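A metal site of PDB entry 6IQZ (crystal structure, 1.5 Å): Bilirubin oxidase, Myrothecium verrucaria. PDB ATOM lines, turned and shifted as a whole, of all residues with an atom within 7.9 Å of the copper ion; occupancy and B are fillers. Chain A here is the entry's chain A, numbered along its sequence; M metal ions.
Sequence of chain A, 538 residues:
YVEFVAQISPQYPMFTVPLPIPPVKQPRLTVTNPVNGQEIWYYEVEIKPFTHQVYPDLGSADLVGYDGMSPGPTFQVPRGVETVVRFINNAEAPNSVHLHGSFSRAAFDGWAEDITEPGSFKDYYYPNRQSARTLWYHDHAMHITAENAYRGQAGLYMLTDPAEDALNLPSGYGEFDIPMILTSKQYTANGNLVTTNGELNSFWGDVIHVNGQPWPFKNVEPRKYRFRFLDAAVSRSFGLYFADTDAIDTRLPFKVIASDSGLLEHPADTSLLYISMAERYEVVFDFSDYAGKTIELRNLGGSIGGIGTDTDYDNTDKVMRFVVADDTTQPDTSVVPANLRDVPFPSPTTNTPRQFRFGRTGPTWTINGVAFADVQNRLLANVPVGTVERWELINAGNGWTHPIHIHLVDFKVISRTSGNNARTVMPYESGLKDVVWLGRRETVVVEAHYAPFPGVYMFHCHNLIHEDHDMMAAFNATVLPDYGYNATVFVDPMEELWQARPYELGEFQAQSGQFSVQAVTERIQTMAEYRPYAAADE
The backbone NH of Met 471 lies within hydrogen-bond range of the backbone carbonyl oxygen of His 466 (2.8 Å).
OD1 of Asn 463 lies within hydrogen-bond range of N of His 466, at 3.5 Å.
O of Asn 201 is in hydrogen-bond range of NE2 of His 466.
The side-chain sulfur (SD) of Met 471 sits close to a ring nitrogen (ND1) of His 402, 3.6 Å away.
O of His 402 is in hydrogen-bond range of N of Leu 438, 2.9 Å away.
The backbone NH (N) of Asn 463 lies close to the side-chain sulfur (SG) of Cys 461.
N of Met 471 is in hydrogen-bond range of O of Trp 365 (3.2 Å).
The backbone NH (N) of Ile 465 sits at hydrogen-bond distance from the side-chain amide oxygen (OD1) of Asn 463 (3.1 Å).
Thr 401 touches the copper ion (O to CU, 3.6 Å).
Asn 463 touches the copper ion.
Met 471 touches the copper ion (SD to CU, 3.4 Å).
Of the 23 residues printed, 6 come within 4 Å of the copper ion.
Along chain A the residues within 4 Å of the copper ion span positions 401 to 471.
The nearest printed residue that does not touch the copper ion is Pro 403 (4.7 Å).
The copper ion is bound by ND1 of His 466, ND1 of His 402 and SG of Cys 461.
The copper ion has three donor atoms within binding distance.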
ATOM      1  N   ASN A 201      11.715 -11.263  23.829  1.00  0.00           N
ATOM      2  CA  ASN A 201      12.674 -11.598  24.890  1.00  0.00           C
ATOM      3  C   ASN A 201      14.078 -11.105  24.542  1.00  0.00           C
ATOM      4  O   ASN A 201      14.610 -10.233  25.210  1.00  0.00           O
ATOM      5  CB  ASN A 201      12.672 -13.118  25.127  1.00  0.00           C
ATOM      6  CG  ASN A 201      13.706 -13.545  26.160  1.00  0.00           C
ATOM      7  OD1 ASN A 201      13.779 -12.988  27.251  1.00  0.00           O
ATOM      8  ND2 ASN A 201      14.522 -14.537  25.800  1.00  0.00           N
ATOM      9  N   SER A 202      14.683 -11.680  23.501  1.00  0.00           N
ATOM     10  CA  SER A 202      15.979 -11.254  22.983  1.00  0.00           C
ATOM     11  C   SER A 202      16.205 -11.904  21.636  1.00  0.00           C
ATOM     12  O   SER A 202      15.792 -13.038  21.405  1.00  0.00           O
ATOM     13  CB  SER A 202      17.134 -11.629  23.920  1.00  0.00           C
ATOM     14  OG  SER A 202      17.339 -10.680  24.954  1.00  0.00           O
ATOM     15  N   MET A 277      26.054  -4.563  24.177  1.00  0.00           N
ATOM     16  CA  MET A 277      25.464  -3.727  23.153  1.00  0.00           C
ATOM     17  C   MET A 277      25.714  -2.246  23.407  1.00  0.00           C
ATOM     18  O   MET A 277      25.484  -1.745  24.528  1.00  0.00           O
ATOM     19  CB  MET A 277      23.956  -3.982  23.039  1.00  0.00           C
ATOM     20  CG  MET A 277      23.566  -5.357  22.464  1.00  0.00           C
ATOM     21  SD  MET A 277      23.826  -6.742  23.602  1.00  0.00           S
ATOM     22  CE  MET A 277      22.434  -6.544  24.719  1.00  0.00           C
ATOM     23  N   PHE A 358      16.018  -2.619  36.734  1.00  0.00           N
ATOM     24  CA  PHE A 358      15.804  -3.064  35.367  1.00  0.00           C
ATOM     25  C   PHE A 358      15.269  -4.481  35.403  1.00  0.00           C
ATOM     26  O   PHE A 358      15.967  -5.416  35.799  1.00  0.00           O
ATOM     27  CB  PHE A 358      17.099  -2.960  34.571  1.00  0.00           C
ATOM     28  CG  PHE A 358      17.599  -1.559  34.488  1.00  0.00           C
ATOM     29  CD1 PHE A 358      18.413  -1.036  35.475  1.00  0.00           C
ATOM     30  CD2 PHE A 358      17.200  -0.730  33.449  1.00  0.00           C
ATOM     31  CE1 PHE A 358      18.840   0.276  35.439  1.00  0.00           C
ATOM     32  CE2 PHE A 358      17.613   0.587  33.396  1.00  0.00           C
ATOM     33  CZ  PHE A 358      18.442   1.095  34.391  1.00  0.00           C
ATOM     34  N   GLY A 359      14.016  -4.651  34.990  1.00  0.00           N
ATOM     35  CA  GLY A 359      13.362  -5.948  35.081  1.00  0.00           C
ATOM     36  C   GLY A 359      12.110  -6.029  34.245  1.00  0.00           C
ATOM     37  O   GLY A 359      11.944  -5.304  33.273  1.00  0.00           O
ATOM     38  N   TRP A 365       9.340  -5.161  29.539  1.00  0.00           N
ATOM     39  CA  TRP A 365      10.622  -4.772  30.103  1.00  0.00           C
ATOM     40  C   TRP A 365      10.500  -3.341  30.603  1.00  0.00           C
ATOM     41  O   TRP A 365      10.080  -2.457  29.860  1.00  0.00           O
ATOM     42  CB  TRP A 365      11.724  -4.914  29.051  1.00  0.00           C
ATOM     43  CG  TRP A 365      11.961  -6.321  28.579  1.00  0.00           C
ATOM     44  CD1 TRP A 365      11.599  -6.864  27.367  1.00  0.00           C
ATOM     45  CD2 TRP A 365      12.613  -7.364  29.310  1.00  0.00           C
ATOM     46  NE1 TRP A 365      12.012  -8.182  27.311  1.00  0.00           N
ATOM     47  CE2 TRP A 365      12.645  -8.512  28.478  1.00  0.00           C
ATOM     48  CE3 TRP A 365      13.204  -7.443  30.577  1.00  0.00           C
ATOM     49  CZ2 TRP A 365      13.198  -9.722  28.888  1.00  0.00           C
ATOM     50  CZ3 TRP A 365      13.764  -8.647  30.981  1.00  0.00           C
ATOM     51  CH2 TRP A 365      13.766  -9.766  30.135  1.00  0.00           C
ATOM     52  N   THR A 366      10.878  -3.104  31.868  1.00  0.00           N
ATOM     53  CA  THR A 366      10.617  -1.811  32.495  1.00  0.00           C
ATOM     54  C   THR A 366      11.793  -1.274  33.306  1.00  0.00           C
ATOM     55  O   THR A 366      12.713  -2.012  33.657  1.00  0.00           O
ATOM     56  CB  THR A 366       9.407  -1.886  33.447  1.00  0.00           C
ATOM     57  OG1 THR A 366       9.611  -2.931  34.407  1.00  0.00           O
ATOM     58  CG2 THR A 366       8.112  -2.157  32.679  1.00  0.00           C
ATOM     59  N   ASN A 395      20.233  -4.882  38.495  1.00  0.00           N
ATOM     60  CA  ASN A 395      19.633  -6.053  37.864  1.00  0.00           C
ATOM     61  C   ASN A 395      19.503  -7.155  38.892  1.00  0.00           C
ATOM     62  O   ASN A 395      20.494  -7.788  39.251  1.00  0.00           O
ATOM     63  CB  ASN A 395      20.477  -6.531  36.679  1.00  0.00           C
ATOM     64  CG  ASN A 395      19.899  -7.770  36.029  1.00  0.00           C
ATOM     65  OD1 ASN A 395      18.728  -8.085  36.228  1.00  0.00           O
ATOM     66  ND2 ASN A 395      20.722  -8.479  35.254  1.00  0.00           N
ATOM     67  N   TRP A 400      18.093 -12.287  32.761  1.00  0.00           N
ATOM     68  CA  TRP A 400      18.351 -11.292  31.727  1.00  0.00           C
ATOM     69  C   TRP A 400      19.579 -10.491  32.106  1.00  0.00           C
ATOM     70  O   TRP A 400      19.988 -10.487  33.273  1.00  0.00           O
ATOM     71  CB  TRP A 400      17.136 -10.354  31.524  1.00  0.00           C
ATOM     72  CG  TRP A 400      16.676  -9.619  32.762  1.00  0.00           C
ATOM     73  CD1 TRP A 400      16.972  -8.321  33.117  1.00  0.00           C
ATOM     74  CD2 TRP A 400      15.852 -10.134  33.819  1.00  0.00           C
ATOM     75  NE1 TRP A 400      16.384  -8.013  34.316  1.00  0.00           N
ATOM     76  CE2 TRP A 400      15.685  -9.098  34.769  1.00  0.00           C
ATOM     77  CE3 TRP A 400      15.231 -11.364  34.049  1.00  0.00           C
ATOM     78  CZ2 TRP A 400      14.948  -9.267  35.928  1.00  0.00           C
ATOM     79  CZ3 TRP A 400      14.489 -11.524  35.208  1.00  0.00           C
ATOM     80  CH2 TRP A 400      14.343 -10.483  36.134  1.00  0.00           C
ATOM     81  N   THR A 401      20.170  -9.835  31.123  1.00  0.00           N
ATOM     82  CA  THR A 401      21.231  -8.855  31.382  1.00  0.00           C
ATOM     83  C   THR A 401      20.933  -7.608  30.560  1.00  0.00           C
ATOM     84  O   THR A 401      20.203  -7.656  29.555  1.00  0.00           O
ATOM     85  CB  THR A 401      22.641  -9.364  31.041  1.00  0.00           C
ATOM     86  OG1 THR A 401      22.825  -9.400  29.615  1.00  0.00           O
ATOM     87  CG2 THR A 401      22.915 -10.728  31.663  1.00  0.00           C
ATOM     88  N   HIS A 402      21.530  -6.489  30.965  1.00  0.00           N
ATOM     89  CA  HIS A 402      21.054  -5.178  30.527  1.00  0.00           C
ATOM     90  C   HIS A 402      22.202  -4.183  30.453  1.00  0.00           C
ATOM     91  O   HIS A 402      22.692  -3.719  31.480  1.00  0.00           O
ATOM     92  CB  HIS A 402      19.987  -4.671  31.497  1.00  0.00           C
ATOM     93  CG  HIS A 402      18.900  -5.664  31.724  1.00  0.00           C
ATOM     94  ND1 HIS A 402      17.876  -5.854  30.821  1.00  0.00           N
ATOM     95  CD2 HIS A 402      18.697  -6.560  32.716  1.00  0.00           C
ATOM     96  CE1 HIS A 402      17.072  -6.814  31.251  1.00  0.00           C
ATOM     97  NE2 HIS A 402      17.554  -7.264  32.398  1.00  0.00           N
ATOM     98  N   PRO A 403      22.630  -3.851  29.239  1.00  0.00           N
ATOM     99  CA  PRO A 403      23.630  -2.791  29.099  1.00  0.00           C
ATOM    100  C   PRO A 403      22.951  -1.424  29.083  1.00  0.00           C
ATOM    101  O   PRO A 403      22.209  -1.126  28.138  1.00  0.00           O
ATOM    102  CB  PRO A 403      24.305  -3.137  27.762  1.00  0.00           C
ATOM    103  CG  PRO A 403      23.254  -3.857  26.964  1.00  0.00           C
ATOM    104  CD  PRO A 403      22.340  -4.534  27.967  1.00  0.00           C
ATOM    105  N   ILE A 404      23.197  -0.629  30.121  1.00  0.00           N
ATOM    106  CA  ILE A 404      22.428   0.588  30.312  1.00  0.00           C
ATOM    107  C   ILE A 404      23.154   1.807  29.769  1.00  0.00           C
ATOM    108  O   ILE A 404      24.314   2.045  30.075  1.00  0.00           O
ATOM    109  CB  ILE A 404      22.134   0.832  31.813  1.00  0.00           C
ATOM    110  CG1 ILE A 404      21.466  -0.403  32.424  1.00  0.00           C
ATOM    111  CG2 ILE A 404      21.275   2.088  31.995  1.00  0.00           C
ATOM    112  CD1 ILE A 404      20.278  -0.903  31.655  1.00  0.00           C
ATOM    113  N   LEU A 438      25.055  -4.519  32.983  1.00  0.00           N
ATOM    114  CA  LEU A 438      24.578  -5.227  34.162  1.00  0.00           C
ATOM    115  C   LEU A 438      24.403  -6.685  33.796  1.00  0.00           C
ATOM    116  O   LEU A 438      23.404  -7.077  33.192  1.00  0.00           O
ATOM    117  CB  LEU A 438      23.247  -4.646  34.676  1.00  0.00           C
ATOM    118  CG  LEU A 438      23.085  -3.135  34.810  1.00  0.00           C
ATOM    119  CD1 LEU A 438      21.715  -2.815  35.405  1.00  0.00           C
ATOM    120  CD2 LEU A 438      24.186  -2.545  35.670  1.00  0.00           C
ATOM    121  N   HIS A 460      18.201   4.099  28.959  1.00  0.00           N
ATOM    122  CA  HIS A 460      17.552   2.859  28.598  1.00  0.00           C
ATOM    123  C   HIS A 460      18.527   1.705  28.529  1.00  0.00           C
ATOM    124  O   HIS A 460      19.736   1.899  28.488  1.00  0.00           O
ATOM    125  CB  HIS A 460      16.858   2.998  27.244  1.00  0.00           C
ATOM    126  CG  HIS A 460      17.789   3.420  26.143  1.00  0.00           C
ATOM    127  ND1 HIS A 460      18.435   2.515  25.333  1.00  0.00           N
ATOM    128  CD2 HIS A 460      18.183   4.648  25.743  1.00  0.00           C
ATOM    129  CE1 HIS A 460      19.187   3.170  24.462  1.00  0.00           C
ATOM    130  NE2 HIS A 460      19.052   4.462  24.693  1.00  0.00           N
ATOM    131  N   CYS A 461      17.973   0.508  28.499  1.00  0.00           N
ATOM    132  CA  CYS A 461      18.747  -0.666  28.134  1.00  0.00           C
ATOM    133  C   CYS A 461      19.032  -0.632  26.663  1.00  0.00           C
ATOM    134  O   CYS A 461      18.168  -0.225  25.880  1.00  0.00           O
ATOM    135  CB  CYS A 461      17.978  -1.931  28.481  1.00  0.00           C
ATOM    136  SG  CYS A 461      18.869  -3.393  28.046  1.00  0.00           S
ATOM    137  N   HIS A 462      20.229  -1.083  26.255  1.00  0.00           N
ATOM    138  CA  HIS A 462      20.578  -1.070  24.837  1.00  0.00           C
ATOM    139  C   HIS A 462      20.509  -2.457  24.182  1.00  0.00           C
ATOM    140  O   HIS A 462      20.968  -2.629  23.062  1.00  0.00           O
ATOM    141  CB  HIS A 462      21.976  -0.475  24.628  1.00  0.00           C
ATOM    142  CG  HIS A 462      22.071   0.440  23.433  1.00  0.00           C
ATOM    143  ND1 HIS A 462      21.995  -0.016  22.136  1.00  0.00           N
ATOM    144  CD2 HIS A 462      22.242   1.780  23.360  1.00  0.00           C
ATOM    145  CE1 HIS A 462      22.131   1.011  21.307  1.00  0.00           C
ATOM    146  NE2 HIS A 462      22.281   2.109  22.024  1.00  0.00           N
ATOM    147  N   ASN A 463      19.909  -3.415  24.876  1.00  0.00           N
ATOM    148  CA  ASN A 463      19.362  -4.597  24.208  1.00  0.00           C
ATOM    149  C   ASN A 463      18.135  -4.097  23.485  1.00  0.00           C
ATOM    150  O   ASN A 463      17.180  -3.678  24.133  1.00  0.00           O
ATOM    151  CB  ASN A 463      19.003  -5.692  25.236  1.00  0.00           C
ATOM    152  CG  ASN A 463      18.434  -6.938  24.595  1.00  0.00           C
ATOM    153  OD1 ASN A 463      17.682  -6.861  23.628  1.00  0.00           O
ATOM    154  ND2 ASN A 463      18.805  -8.098  25.119  1.00  0.00           N
ATOM    155  N   LEU A 464      18.163  -4.087  22.150  1.00  0.00           N
ATOM    156  CA  LEU A 464      17.146  -3.343  21.433  1.00  0.00           C
ATOM    157  C   LEU A 464      15.765  -3.989  21.531  1.00  0.00           C
ATOM    158  O   LEU A 464      14.763  -3.289  21.391  1.00  0.00           O
ATOM    159  CB  LEU A 464      17.556  -3.180  19.972  1.00  0.00           C
ATOM    160  CG  LEU A 464      18.888  -2.484  19.772  1.00  0.00           C
ATOM    161  CD1 LEU A 464      19.128  -2.285  18.285  1.00  0.00           C
ATOM    162  CD2 LEU A 464      18.893  -1.158  20.497  1.00  0.00           C
ATOM    163  N   ILE A 465      15.707  -5.284  21.778  1.00  0.00           N
ATOM    164  CA  ILE A 465      14.423  -5.942  22.047  1.00  0.00           C
ATOM    165  C   ILE A 465      13.833  -5.432  23.371  1.00  0.00           C
ATOM    166  O   ILE A 465      12.652  -5.096  23.454  1.00  0.00           O
ATOM    167  CB  ILE A 465      14.568  -7.480  22.088  1.00  0.00           C
ATOM    168  CG1 ILE A 465      15.045  -8.014  20.736  1.00  0.00           C
ATOM    169  CG2 ILE A 465      13.250  -8.150  22.480  1.00  0.00           C
ATOM    170  CD1 ILE A 465      14.106  -7.693  19.565  1.00  0.00           C
ATOM    171  N   HIS A 466      14.677  -5.311  24.393  1.00  0.00           N
ATOM    172  CA  HIS A 466      14.199  -4.796  25.681  1.00  0.00           C
ATOM    173  C   HIS A 466      13.768  -3.351  25.533  1.00  0.00           C
ATOM    174  O   HIS A 466      12.723  -2.944  26.057  1.00  0.00           O
ATOM    175  CB  HIS A 466      15.291  -4.877  26.752  1.00  0.00           C
ATOM    176  CG  HIS A 466      15.744  -6.275  27.062  1.00  0.00           C
ATOM    177  ND1 HIS A 466      16.773  -6.546  27.923  1.00  0.00           N
ATOM    178  CD2 HIS A 466      15.299  -7.483  26.624  1.00  0.00           C
ATOM    179  CE1 HIS A 466      16.962  -7.855  28.001  1.00  0.00           C
ATOM    180  NE2 HIS A 466      16.069  -8.437  27.229  1.00  0.00           N
ATOM    181  N   GLU A 467      14.596  -2.579  24.837  1.00  0.00           N
ATOM    182  CA  GLU A 467      14.338  -1.159  24.629  1.00  0.00           C
ATOM    183  C   GLU A 467      12.979  -0.918  23.954  1.00  0.00           C
ATOM    184  O   GLU A 467      12.235  -0.025  24.337  1.00  0.00           O
ATOM    185  CB  GLU A 467      15.484  -0.551  23.812  1.00  0.00           C
ATOM    186  CG  GLU A 467      15.355   0.935  23.534  1.00  0.00           C
ATOM    187  CD  GLU A 467      16.501   1.450  22.681  1.00  0.00           C
ATOM    188  OE1 GLU A 467      17.601   0.857  22.746  1.00  0.00           O
ATOM    189  OE2 GLU A 467      16.301   2.431  21.930  1.00  0.00           O
ATOM    190  N   MET A 471      11.842  -0.824  27.741  1.00  0.00           N
ATOM    191  CA  MET A 471      12.767  -0.502  28.846  1.00  0.00           C
ATOM    192  C   MET A 471      13.527   0.784  28.589  1.00  0.00           C
ATOM    193  O   MET A 471      14.746   0.786  28.360  1.00  0.00           O
ATOM    194  CB  MET A 471      13.750  -1.664  29.049  1.00  0.00           C
ATOM    195  CG  MET A 471      14.555  -1.618  30.348  1.00  0.00           C
ATOM    196  SD  MET A 471      15.575  -3.100  30.517  1.00  0.00           S
ATOM    197  CE  MET A 471      14.640  -4.014  31.736  1.00  0.00           C
HETATM  198 CU    CU M   1      17.799  -5.057  28.916  1.00  0.00          CU
